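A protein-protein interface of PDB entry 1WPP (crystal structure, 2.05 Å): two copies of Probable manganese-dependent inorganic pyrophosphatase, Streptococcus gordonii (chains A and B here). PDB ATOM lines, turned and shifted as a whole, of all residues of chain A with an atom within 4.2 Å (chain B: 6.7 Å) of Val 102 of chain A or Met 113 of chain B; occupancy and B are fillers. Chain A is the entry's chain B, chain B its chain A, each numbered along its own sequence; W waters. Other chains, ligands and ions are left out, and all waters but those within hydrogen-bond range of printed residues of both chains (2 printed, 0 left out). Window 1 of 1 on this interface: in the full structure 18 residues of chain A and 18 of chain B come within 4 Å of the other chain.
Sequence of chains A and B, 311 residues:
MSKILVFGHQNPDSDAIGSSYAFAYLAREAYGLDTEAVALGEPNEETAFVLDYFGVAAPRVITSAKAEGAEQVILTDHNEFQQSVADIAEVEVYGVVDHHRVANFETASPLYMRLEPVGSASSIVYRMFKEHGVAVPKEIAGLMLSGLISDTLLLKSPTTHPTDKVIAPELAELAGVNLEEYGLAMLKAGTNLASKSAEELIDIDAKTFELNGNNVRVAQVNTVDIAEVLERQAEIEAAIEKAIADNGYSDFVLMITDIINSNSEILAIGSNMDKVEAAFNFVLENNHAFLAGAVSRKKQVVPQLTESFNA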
ATOM      1  N   ASN A  79       2.339 -15.481  17.481  1.00  0.00           N
ATOM      2  CA  ASN A  79       3.449 -16.415  17.307  1.00  0.00           C
ATOM      3  C   ASN A  79       2.881 -17.851  17.318  1.00  0.00           C
ATOM      4  O   ASN A  79       3.479 -18.779  16.768  1.00  0.00           O
ATOM      5  CB  ASN A  79       4.476 -16.231  18.419  1.00  0.00           C
ATOM      6  CG  ASN A  79       3.858 -16.408  19.806  1.00  0.00           C
ATOM      7  OD1 ASN A  79       3.823 -17.534  20.353  1.00  0.00           O
ATOM      8  ND2 ASN A  79       3.359 -15.310  20.386  1.00  0.00           N
ATOM      9  N   HIS A 100       1.804 -10.792  22.634  1.00  0.00           N
ATOM     10  CA  HIS A 100       1.093 -11.884  23.331  1.00  0.00           C
ATOM     11  C   HIS A 100       2.042 -12.826  24.047  1.00  0.00           C
ATOM     12  O   HIS A 100       3.249 -12.734  23.905  1.00  0.00           O
ATOM     13  CB  HIS A 100       0.191 -12.709  22.370  1.00  0.00           C
ATOM     14  CG  HIS A 100      -0.851 -11.889  21.682  1.00  0.00           C
ATOM     15  ND1 HIS A 100      -0.634 -11.292  20.455  1.00  0.00           N
ATOM     16  CD2 HIS A 100      -2.081 -11.496  22.084  1.00  0.00           C
ATOM     17  CE1 HIS A 100      -1.703 -10.600  20.117  1.00  0.00           C
ATOM     18  NE2 HIS A 100      -2.606 -10.731  21.076  1.00  0.00           N
ATOM     19  N   ARG A 101       1.489 -13.753  24.826  1.00  0.00           N
ATOM     20  CA  ARG A 101       2.271 -14.858  25.378  1.00  0.00           C
ATOM     21  C   ARG A 101       2.811 -15.762  24.252  1.00  0.00           C
ATOM     22  O   ARG A 101       2.267 -15.803  23.164  1.00  0.00           O
ATOM     23  CB  ARG A 101       1.415 -15.678  26.364  1.00  0.00           C
ATOM     24  CG  ARG A 101       0.156 -16.408  25.810  1.00  0.00           C
ATOM     25  CD  ARG A 101       0.439 -17.803  25.267  1.00  0.00           C
ATOM     26  NE  ARG A 101      -0.706 -18.706  25.183  1.00  0.00           N
ATOM     27  CZ  ARG A 101      -0.930 -19.730  26.014  1.00  0.00           C
ATOM     28  NH1 ARG A 101      -0.119 -19.980  27.046  1.00  0.00           N
ATOM     29  NH2 ARG A 101      -1.986 -20.501  25.820  1.00  0.00           N
ATOM     30  N   VAL A 102       3.826 -16.560  24.572  1.00  0.00           N
ATOM     31  CA  VAL A 102       4.451 -17.441  23.586  1.00  0.00           C
ATOM     32  C   VAL A 102       3.967 -18.835  23.900  1.00  0.00           C
ATOM     33  O   VAL A 102       4.089 -19.284  25.040  1.00  0.00           O
ATOM     34  CB  VAL A 102       5.996 -17.348  23.656  1.00  0.00           C
ATOM     35  CG1 VAL A 102       6.719 -18.373  22.737  1.00  0.00           C
ATOM     36  CG2 VAL A 102       6.423 -15.949  23.307  1.00  0.00           C
ATOM     37  N   ALA A 103       3.437 -19.524  22.890  1.00  0.00           N
ATOM     38  CA  ALA A 103       3.018 -20.935  23.043  1.00  0.00           C
ATOM     39  C   ALA A 103       2.907 -21.494  21.650  1.00  0.00           C
ATOM     40  O   ALA A 103       2.821 -20.731  20.683  1.00  0.00           O
ATOM     41  CB  ALA A 103       1.639 -21.059  23.749  1.00  0.00           C
ATOM     42  N   MET A 113      13.363 -11.768  17.277  1.00  0.00           N
ATOM     43  CA  MET A 113      12.085 -11.581  17.951  1.00  0.00           C
ATOM     44  C   MET A 113      12.133 -10.257  18.714  1.00  0.00           C
ATOM     45  O   MET A 113      13.112  -9.938  19.374  1.00  0.00           O
ATOM     46  CB  MET A 113      11.751 -12.722  18.939  1.00  0.00           C
ATOM     47  CG  MET A 113      11.569 -14.084  18.311  1.00  0.00           C
ATOM     48  SD  MET A 113      11.126 -15.441  19.465  1.00  0.00           S
ATOM     49  CE  MET A 113       9.319 -15.387  19.564  1.00  0.00           C
ATOM     50  N   ARG A 114      11.047  -9.508  18.603  1.00  0.00           N
ATOM     51  CA  ARG A 114      10.826  -8.329  19.402  1.00  0.00           C
ATOM     52  C   ARG A 114       9.441  -8.455  20.023  1.00  0.00           C
ATOM     53  O   ARG A 114       8.433  -8.282  19.341  1.00  0.00           O
ATOM     54  CB  ARG A 114      10.905  -7.066  18.537  1.00  0.00           C
ATOM     55  CG  ARG A 114      11.114  -5.806  19.349  1.00  0.00           C
ATOM     56  CD  ARG A 114      12.553  -5.592  19.751  1.00  0.00           C
ATOM     57  NE  ARG A 114      13.432  -5.537  18.582  1.00  0.00           N
ATOM     58  CZ  ARG A 114      14.191  -4.493  18.283  1.00  0.00           C
ATOM     59  NH1 ARG A 114      14.946  -4.521  17.214  1.00  0.00           N
ATOM     60  NH2 ARG A 114      14.171  -3.410  19.057  1.00  0.00           N
ATOM     61  N   LEU A 115       9.400  -8.775  21.313  1.00  0.00           N
ATOM     62  CA  LEU A 115       8.145  -8.946  22.012  1.00  0.00           C
ATOM     63  C   LEU A 115       8.208  -7.981  23.184  1.00  0.00           C
ATOM     64  O   LEU A 115       9.304  -7.750  23.751  1.00  0.00           O
ATOM     65  CB  LEU A 115       8.024 -10.370  22.524  1.00  0.00           C
ATOM     66  CG  LEU A 115       7.134 -11.250  21.645  1.00  0.00           C
ATOM     67  CD1 LEU A 115       7.866 -11.612  20.305  1.00  0.00           C
ATOM     68  CD2 LEU A 115       6.777 -12.534  22.346  1.00  0.00           C
ATOM     69  N   ASN B  79      16.710 -19.848  26.272  1.00  0.00           N
ATOM     70  CA  ASN B  79      15.277 -19.798  26.555  1.00  0.00           C
ATOM     71  C   ASN B  79      14.724 -21.178  26.853  1.00  0.00           C
ATOM     72  O   ASN B  79      13.664 -21.290  27.488  1.00  0.00           O
ATOM     73  CB  ASN B  79      14.483 -19.205  25.353  1.00  0.00           C
ATOM     74  CG  ASN B  79      14.653 -20.022  24.071  1.00  0.00           C
ATOM     75  OD1 ASN B  79      13.867 -20.934  23.777  1.00  0.00           O
ATOM     76  ND2 ASN B  79      15.684 -19.712  23.318  1.00  0.00           N
ATOM     77  N   TYR B  94       9.844 -12.714  32.911  1.00  0.00           N
ATOM     78  CA  TYR B  94       9.594 -11.306  32.648  1.00  0.00           C
ATOM     79  C   TYR B  94      10.211 -10.992  31.288  1.00  0.00           C
ATOM     80  O   TYR B  94       9.675 -10.196  30.508  1.00  0.00           O
ATOM     81  CB  TYR B  94      10.273 -10.452  33.723  1.00  0.00           C
ATOM     82  CG  TYR B  94       9.981  -8.954  33.644  1.00  0.00           C
ATOM     83  CD1 TYR B  94       8.900  -8.364  34.360  1.00  0.00           C
ATOM     84  CD2 TYR B  94      10.790  -8.126  32.897  1.00  0.00           C
ATOM     85  CE1 TYR B  94       8.646  -6.945  34.271  1.00  0.00           C
ATOM     86  CE2 TYR B  94      10.551  -6.754  32.801  1.00  0.00           C
ATOM     87  CZ  TYR B  94       9.504  -6.163  33.479  1.00  0.00           C
ATOM     88  OH  TYR B  94       9.378  -4.786  33.322  1.00  0.00           O
ATOM     89  N   GLY B  95      11.344 -11.616  31.002  1.00  0.00           N
ATOM     90  CA  GLY B  95      12.038 -11.251  29.771  1.00  0.00           C
ATOM     91  C   GLY B  95      13.119 -12.178  29.336  1.00  0.00           C
ATOM     92  O   GLY B  95      13.630 -12.943  30.133  1.00  0.00           O
ATOM     93  N   VAL B  96      13.456 -12.146  28.045  1.00  0.00           N
ATOM     94  CA  VAL B  96      14.462 -13.036  27.498  1.00  0.00           C
ATOM     95  C   VAL B  96      15.297 -12.245  26.481  1.00  0.00           C
ATOM     96  O   VAL B  96      14.716 -11.613  25.616  1.00  0.00           O
ATOM     97  CB  VAL B  96      13.874 -14.240  26.686  1.00  0.00           C
ATOM     98  CG1 VAL B  96      15.030 -15.058  26.105  1.00  0.00           C
ATOM     99  CG2 VAL B  96      12.976 -15.127  27.532  1.00  0.00           C
ATOM    100  N   VAL B  97      16.619 -12.302  26.592  1.00  0.00           N
ATOM    101  CA  VAL B  97      17.565 -11.771  25.594  1.00  0.00           C
ATOM    102  C   VAL B  97      18.424 -12.927  25.079  1.00  0.00           C
ATOM    103  O   VAL B  97      19.198 -13.528  25.820  1.00  0.00           O
ATOM    104  CB  VAL B  97      18.474 -10.614  26.160  1.00  0.00           C
ATOM    105  CG1 VAL B  97      19.435 -10.060  25.081  1.00  0.00           C
ATOM    106  CG2 VAL B  97      17.587  -9.474  26.669  1.00  0.00           C
ATOM    107  N   ASP B  98      18.267 -13.320  23.828  1.00  0.00           N
ATOM    108  CA  ASP B  98      18.980 -14.521  23.419  1.00  0.00           C
ATOM    109  C   ASP B  98      19.371 -14.460  21.933  1.00  0.00           C
ATOM    110  O   ASP B  98      18.930 -13.543  21.237  1.00  0.00           O
ATOM    111  CB  ASP B  98      18.098 -15.736  23.739  1.00  0.00           C
ATOM    112  CG  ASP B  98      18.848 -17.043  23.647  1.00  0.00           C
ATOM    113  OD1 ASP B  98      18.177 -18.093  23.531  1.00  0.00           O
ATOM    114  OD2 ASP B  98      20.099 -17.104  23.674  1.00  0.00           O
ATOM    115  N   VAL B 102      14.354 -21.099  19.335  1.00  0.00           N
ATOM    116  CA  VAL B 102      13.430 -21.111  20.438  1.00  0.00           C
ATOM    117  C   VAL B 102      12.762 -22.503  20.467  1.00  0.00           C
ATOM    118  O   VAL B 102      12.235 -22.975  19.450  1.00  0.00           O
ATOM    119  CB  VAL B 102      12.347 -20.042  20.251  1.00  0.00           C
ATOM    120  CG1 VAL B 102      11.309 -20.129  21.351  1.00  0.00           C
ATOM    121  CG2 VAL B 102      12.938 -18.679  20.248  1.00  0.00           C
ATOM    122  N   PHE B 105       9.869 -23.782  25.331  1.00  0.00           N
ATOM    123  CA  PHE B 105       9.701 -22.498  25.980  1.00  0.00           C
ATOM    124  C   PHE B 105       8.283 -22.046  25.766  1.00  0.00           C
ATOM    125  O   PHE B 105       7.777 -22.077  24.629  1.00  0.00           O
ATOM    126  CB  PHE B 105      10.694 -21.470  25.399  1.00  0.00           C
ATOM    127  CG  PHE B 105      10.479 -20.043  25.928  1.00  0.00           C
ATOM    128  CD1 PHE B 105       9.696 -19.135  25.231  1.00  0.00           C
ATOM    129  CD2 PHE B 105      11.018 -19.650  27.163  1.00  0.00           C
ATOM    130  CE1 PHE B 105       9.471 -17.804  25.713  1.00  0.00           C
ATOM    131  CE2 PHE B 105      10.804 -18.338  27.656  1.00  0.00           C
ATOM    132  CZ  PHE B 105      10.019 -17.427  26.910  1.00  0.00           C
ATOM    133  N   GLU B 106       7.661 -21.561  26.824  1.00  0.00           N
ATOM    134  CA  GLU B 106       6.252 -21.215  26.806  1.00  0.00           C
ATOM    135  C   GLU B 106       5.962 -20.259  27.964  1.00  0.00           C
ATOM    136  O   GLU B 106       6.630 -20.346  28.991  1.00  0.00           O
ATOM    137  CB  GLU B 106       5.445 -22.478  27.058  1.00  0.00           C
ATOM    138  CG  GLU B 106       4.039 -22.401  26.569  1.00  0.00           C
ATOM    139  CD  GLU B 106       3.211 -23.583  27.034  1.00  0.00           C
ATOM    140  OE1 GLU B 106       2.014 -23.550  26.713  1.00  0.00           O
ATOM    141  OE2 GLU B 106       3.747 -24.513  27.729  1.00  0.00           O
ATOM    142  N   THR B 107       5.003 -19.338  27.795  1.00  0.00           N
ATOM    143  CA  THR B 107       4.550 -18.469  28.879  1.00  0.00           C
ATOM    144  C   THR B 107       3.045 -18.393  28.900  1.00  0.00           C
ATOM    145  O   THR B 107       2.390 -18.635  27.883  1.00  0.00           O
ATOM    146  CB  THR B 107       5.107 -17.008  28.759  1.00  0.00           C
ATOM    147  OG1 THR B 107       4.526 -16.352  27.608  1.00  0.00           O
ATOM    148  CG2 THR B 107       6.636 -16.983  28.529  1.00  0.00           C
ATOM    149  N   ALA B 108       2.510 -18.011  30.052  1.00  0.00           N
ATOM    150  CA  ALA B 108       1.071 -17.847  30.256  1.00  0.00           C
ATOM    151  C   ALA B 108       0.662 -16.420  29.900  1.00  0.00           C
ATOM    152  O   ALA B 108      -0.478 -16.178  29.512  1.00  0.00           O
ATOM    153  CB  ALA B 108       0.709 -18.125  31.726  1.00  0.00           C
ATOM    154  N   SER B 109       1.590 -15.480  30.088  1.00  0.00           N
ATOM    155  CA  SER B 109       1.306 -14.042  29.944  1.00  0.00           C
ATOM    156  C   SER B 109       2.328 -13.435  28.959  1.00  0.00           C
ATOM    157  O   SER B 109       3.378 -14.036  28.750  1.00  0.00           O
ATOM    158  CB  SER B 109       1.420 -13.354  31.310  1.00  0.00           C
ATOM    159  OG  SER B 109       0.680 -14.049  32.309  1.00  0.00           O
ATOM    160  N   PRO B 110       2.033 -12.284  28.341  1.00  0.00           N
ATOM    161  CA  PRO B 110       3.042 -11.565  27.536  1.00  0.00           C
ATOM    162  C   PRO B 110       4.343 -11.273  28.274  1.00  0.00           C
ATOM    163  O   PRO B 110       4.361 -11.273  29.511  1.00  0.00           O
ATOM    164  CB  PRO B 110       2.340 -10.243  27.204  1.00  0.00           C
ATOM    165  CG  PRO B 110       0.867 -10.624  27.112  1.00  0.00           C
ATOM    166  CD  PRO B 110       0.718 -11.590  28.286  1.00  0.00           C
ATOM    167  N   LEU B 111       5.423 -11.000  27.534  1.00  0.00           N
ATOM    168  CA  LEU B 111       6.712 -10.732  28.187  1.00  0.00           C
ATOM    169  C   LEU B 111       7.537  -9.866  27.254  1.00  0.00           C
ATOM    170  O   LEU B 111       7.061  -9.549  26.130  1.00  0.00           O
ATOM    171  CB  LEU B 111       7.447 -12.086  28.449  1.00  0.00           C
ATOM    172  CG  LEU B 111       7.986 -12.835  27.215  1.00  0.00           C
ATOM    173  CD1 LEU B 111       9.060 -13.840  27.670  1.00  0.00           C
ATOM    174  CD2 LEU B 111       6.910 -13.547  26.347  1.00  0.00           C
ATOM    175  N   TYR B 112       8.752  -9.499  27.682  1.00  0.00           N
ATOM    176  CA  TYR B 112       9.720  -8.919  26.775  1.00  0.00           C
ATOM    177  C   TYR B 112      10.562 -10.047  26.166  1.00  0.00           C
ATOM    178  O   TYR B 112      11.057 -10.907  26.897  1.00  0.00           O
ATOM    179  CB  TYR B 112      10.679  -7.975  27.513  1.00  0.00           C
ATOM    180  CG  TYR B 112      10.054  -6.676  27.976  1.00  0.00           C
ATOM    181  CD1 TYR B 112       9.992  -5.579  27.125  1.00  0.00           C
ATOM    182  CD2 TYR B 112       9.500  -6.545  29.275  1.00  0.00           C
ATOM    183  CE1 TYR B 112       9.420  -4.348  27.562  1.00  0.00           C
ATOM    184  CE2 TYR B 112       8.919  -5.331  29.706  1.00  0.00           C
ATOM    185  CZ  TYR B 112       8.897  -4.238  28.828  1.00  0.00           C
ATOM    186  OH  TYR B 112       8.302  -3.032  29.177  1.00  0.00           O
ATOM    187  N   MET B 113      10.756 -10.034  24.849  1.00  0.00           N
ATOM    188  CA  MET B 113      11.789 -10.874  24.225  1.00  0.00           C
ATOM    189  C   MET B 113      12.555 -10.027  23.240  1.00  0.00           C
ATOM    190  O   MET B 113      11.971  -9.301  22.484  1.00  0.00           O
ATOM    191  CB  MET B 113      11.226 -12.079  23.470  1.00  0.00           C
ATOM    192  CG  MET B 113      10.439 -13.033  24.362  1.00  0.00           C
ATOM    193  SD  MET B 113       9.938 -14.559  23.578  1.00  0.00           S
ATOM    194  CE  MET B 113      11.434 -15.483  23.583  1.00  0.00           C
ATOM    195  N   ARG B 114      13.876 -10.131  23.283  1.00  0.00           N
ATOM    196  CA  ARG B 114      14.724  -9.494  22.300  1.00  0.00           C
ATOM    197  C   ARG B 114      15.698 -10.541  21.804  1.00  0.00           C
ATOM    198  O   ARG B 114      16.729 -10.803  22.443  1.00  0.00           O
ATOM    199  CB  ARG B 114      15.499  -8.324  22.897  1.00  0.00           C
ATOM    200  CG  ARG B 114      16.330  -7.596  21.843  1.00  0.00           C
ATOM    201  CD  ARG B 114      15.610  -6.487  21.108  1.00  0.00           C
ATOM    202  NE  ARG B 114      14.796  -5.695  22.014  1.00  0.00           N
ATOM    203  CZ  ARG B 114      14.939  -4.390  22.183  1.00  0.00           C
ATOM    204  NH1 ARG B 114      15.868  -3.734  21.509  1.00  0.00           N
ATOM    205  NH2 ARG B 114      14.155  -3.745  23.021  1.00  0.00           N
ATOM    206  N   LEU B 115      15.374 -11.144  20.661  1.00  0.00           N
ATOM    207  CA  LEU B 115      16.250 -12.153  20.070  1.00  0.00           C
ATOM    208  C   LEU B 115      16.797 -11.676  18.727  1.00  0.00           C
ATOM    209  O   LEU B 115      16.082 -11.025  17.931  1.00  0.00           O
ATOM    210  CB  LEU B 115      15.492 -13.507  19.923  1.00  0.00           C
ATOM    211  CG  LEU B 115      15.593 -14.512  21.080  1.00  0.00           C
ATOM    212  CD1 LEU B 115      14.956 -14.024  22.386  1.00  0.00           C
ATOM    213  CD2 LEU B 115      14.898 -15.832  20.682  1.00  0.00           C
HETATM  214  O   HOH W   1      14.568  -8.203  17.702  1.00  0.00           O
HETATM  215  O   HOH W   2       4.515 -10.487  24.735  1.00  0.00           O
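Among the printed residues, pairs that only touch across the chains: Leu 115 of chain A with Tyr 112 of chain B (3.3 Å), Met 113 of chain A with Arg 114 of chain B (3.4 Å), Val 102 of chain A with Glu 106 of chain B (3.4 Å), Arg 114 of chain A with Met 113 of chain B (3.4 Å), Arg 101 of chain A with Ser 109 of chain B (3.5 Å), Leu 115 of chain A with Leu 111 of chain B (3.5 Å), Arg 101 of chain A with Ala 108 of chain B (3.7 Å), Val 102 of chain A with Met 113 of chain B (3.8 Å), Met 113 of chain A with Val 102 of chain B (3.8 Å), Arg 101 of chain A with Pro 110 of chain B (3.8 Å), His 100 of chain A with Pro 110 of chain B (3.8 Å), Ala 103 of chain A with Glu 106 of chain B (3.9 Å), Val 102 of chain A with Leu 111 of chain B (3.9 Å) and Val 102 of chain A with Phe 105 of chain B (3.96 Å).
Val 102 of chain A touches Met 113 of chain B, and with the chains exchanged Met 113 of chain A touches Val 102 of chain B. Met 113 of chain A touches Arg 114 of chain B, and with the chains exchanged Arg 114 of chain A touches Met 113 of chain B. Met 113 of chain A touches Leu 115 of chain B, and with the chains exchanged Leu 115 of chain A touches Met 113 of chain B. Arg 114 of chain B touches its own counterpart, Arg 114 of chain A. Of the 20 pairs that touch across the chains among the printed residues, 8 have their exchanged pair printed and touching as well.
O of Tyr 112 of chain B is in hydrogen-bond range of N of Val 96 of chain B (2.9 Å). The backbone carbonyl oxygen (O) of Val 96 of chain B lies within hydrogen-bond range of the backbone NH (N) of Arg 114 of chain B (2.9 Å). N of Asp 98 of chain B is in hydrogen-bond range of O of Arg 114 of chain B. The side-chain hydroxyl (OG1) of Thr 107 of chain B lies within hydrogen-bond range of the backbone carbonyl oxygen (O) of Ser 109 of chain B (2.8 Å). O of Tyr 94 of chain B is in hydrogen-bond range of N of Tyr 112 of chain B (3.1 Å). ND2 of Asn 79 of chain A is in hydrogen-bond range of O of Arg 101 of chain A, 3.0 Å away.
Of the printed residues of chain B, His 100 of chain A touches Pro 110 (3.8 Å). Val 102 of chain A touches just these residues of chain B: Phe 105, Glu 106, Thr 107, Leu 111 and Met 113. Val 97 of chain B touches none of the printed residues of chain A. Of the printed residues of chain A, Ala 108 of chain B touches Arg 101. Of the printed residues of chain A, Leu 111 of chain B touches Val 102 and Leu 115. Of the printed residues of chain A, Met 113 of chain B touches Val 102 (3.8 Å), Met 113 (3.4 Å), Arg 114 (3.4 Å) and Leu 115 (2.9 Å).
Hydrophobic or aromatic side chains of chain B within 4 Å of the printed part of chain A: Val 102, Phe 105, Pro 110, Leu 111, Met 113 and Leu 115. Among the printed residues, 20 pairs touch across the chains. Among the printed residues, no Asp or Glu carboxylate lies within 4 Å of a Lys or Arg side-chain nitrogen of the other chain.
Water W2 lies within hydrogen-bond range of the backbone carbonyl oxygen (O) of His 100 of chain A (2.7 Å) and the backbone NH (N) of Leu 111 of chain B (3.0 Å). Water W1 lies within hydrogen-bond range of O of Met 113 of chain A (2.8 Å), NE of Arg 114 of chain A (3.0 Å) and O of Leu 115 of chain B (3.2 Å).
O of Met 113 of chain A sits close to O of Met 113 of chain B (3.4 Å). The guanidinium group of Arg 114 of chain A sits close to the guanidinium group of Arg 114 of chain B (3.0 Å). The guanidinium group (NH1) of Arg 101 of chain A sits at hydrogen-bond distance from the backbone carbonyl oxygen (O) of Thr 107 of chain B. N of Leu 115 of chain B sits at hydrogen-bond distance from O of Met 113 of chain A, at 2.9 Å. The backbone carbonyl oxygen of Met 113 of chain B sits at hydrogen-bond distance from the backbone NH of Leu 115 of chain A, 2.9 Å away. The backbone NH (N) of Thr 107 of chain B is in hydrogen-bond range of the backbone carbonyl oxygen (O) of Val 102 of chain A (2.9 Å).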
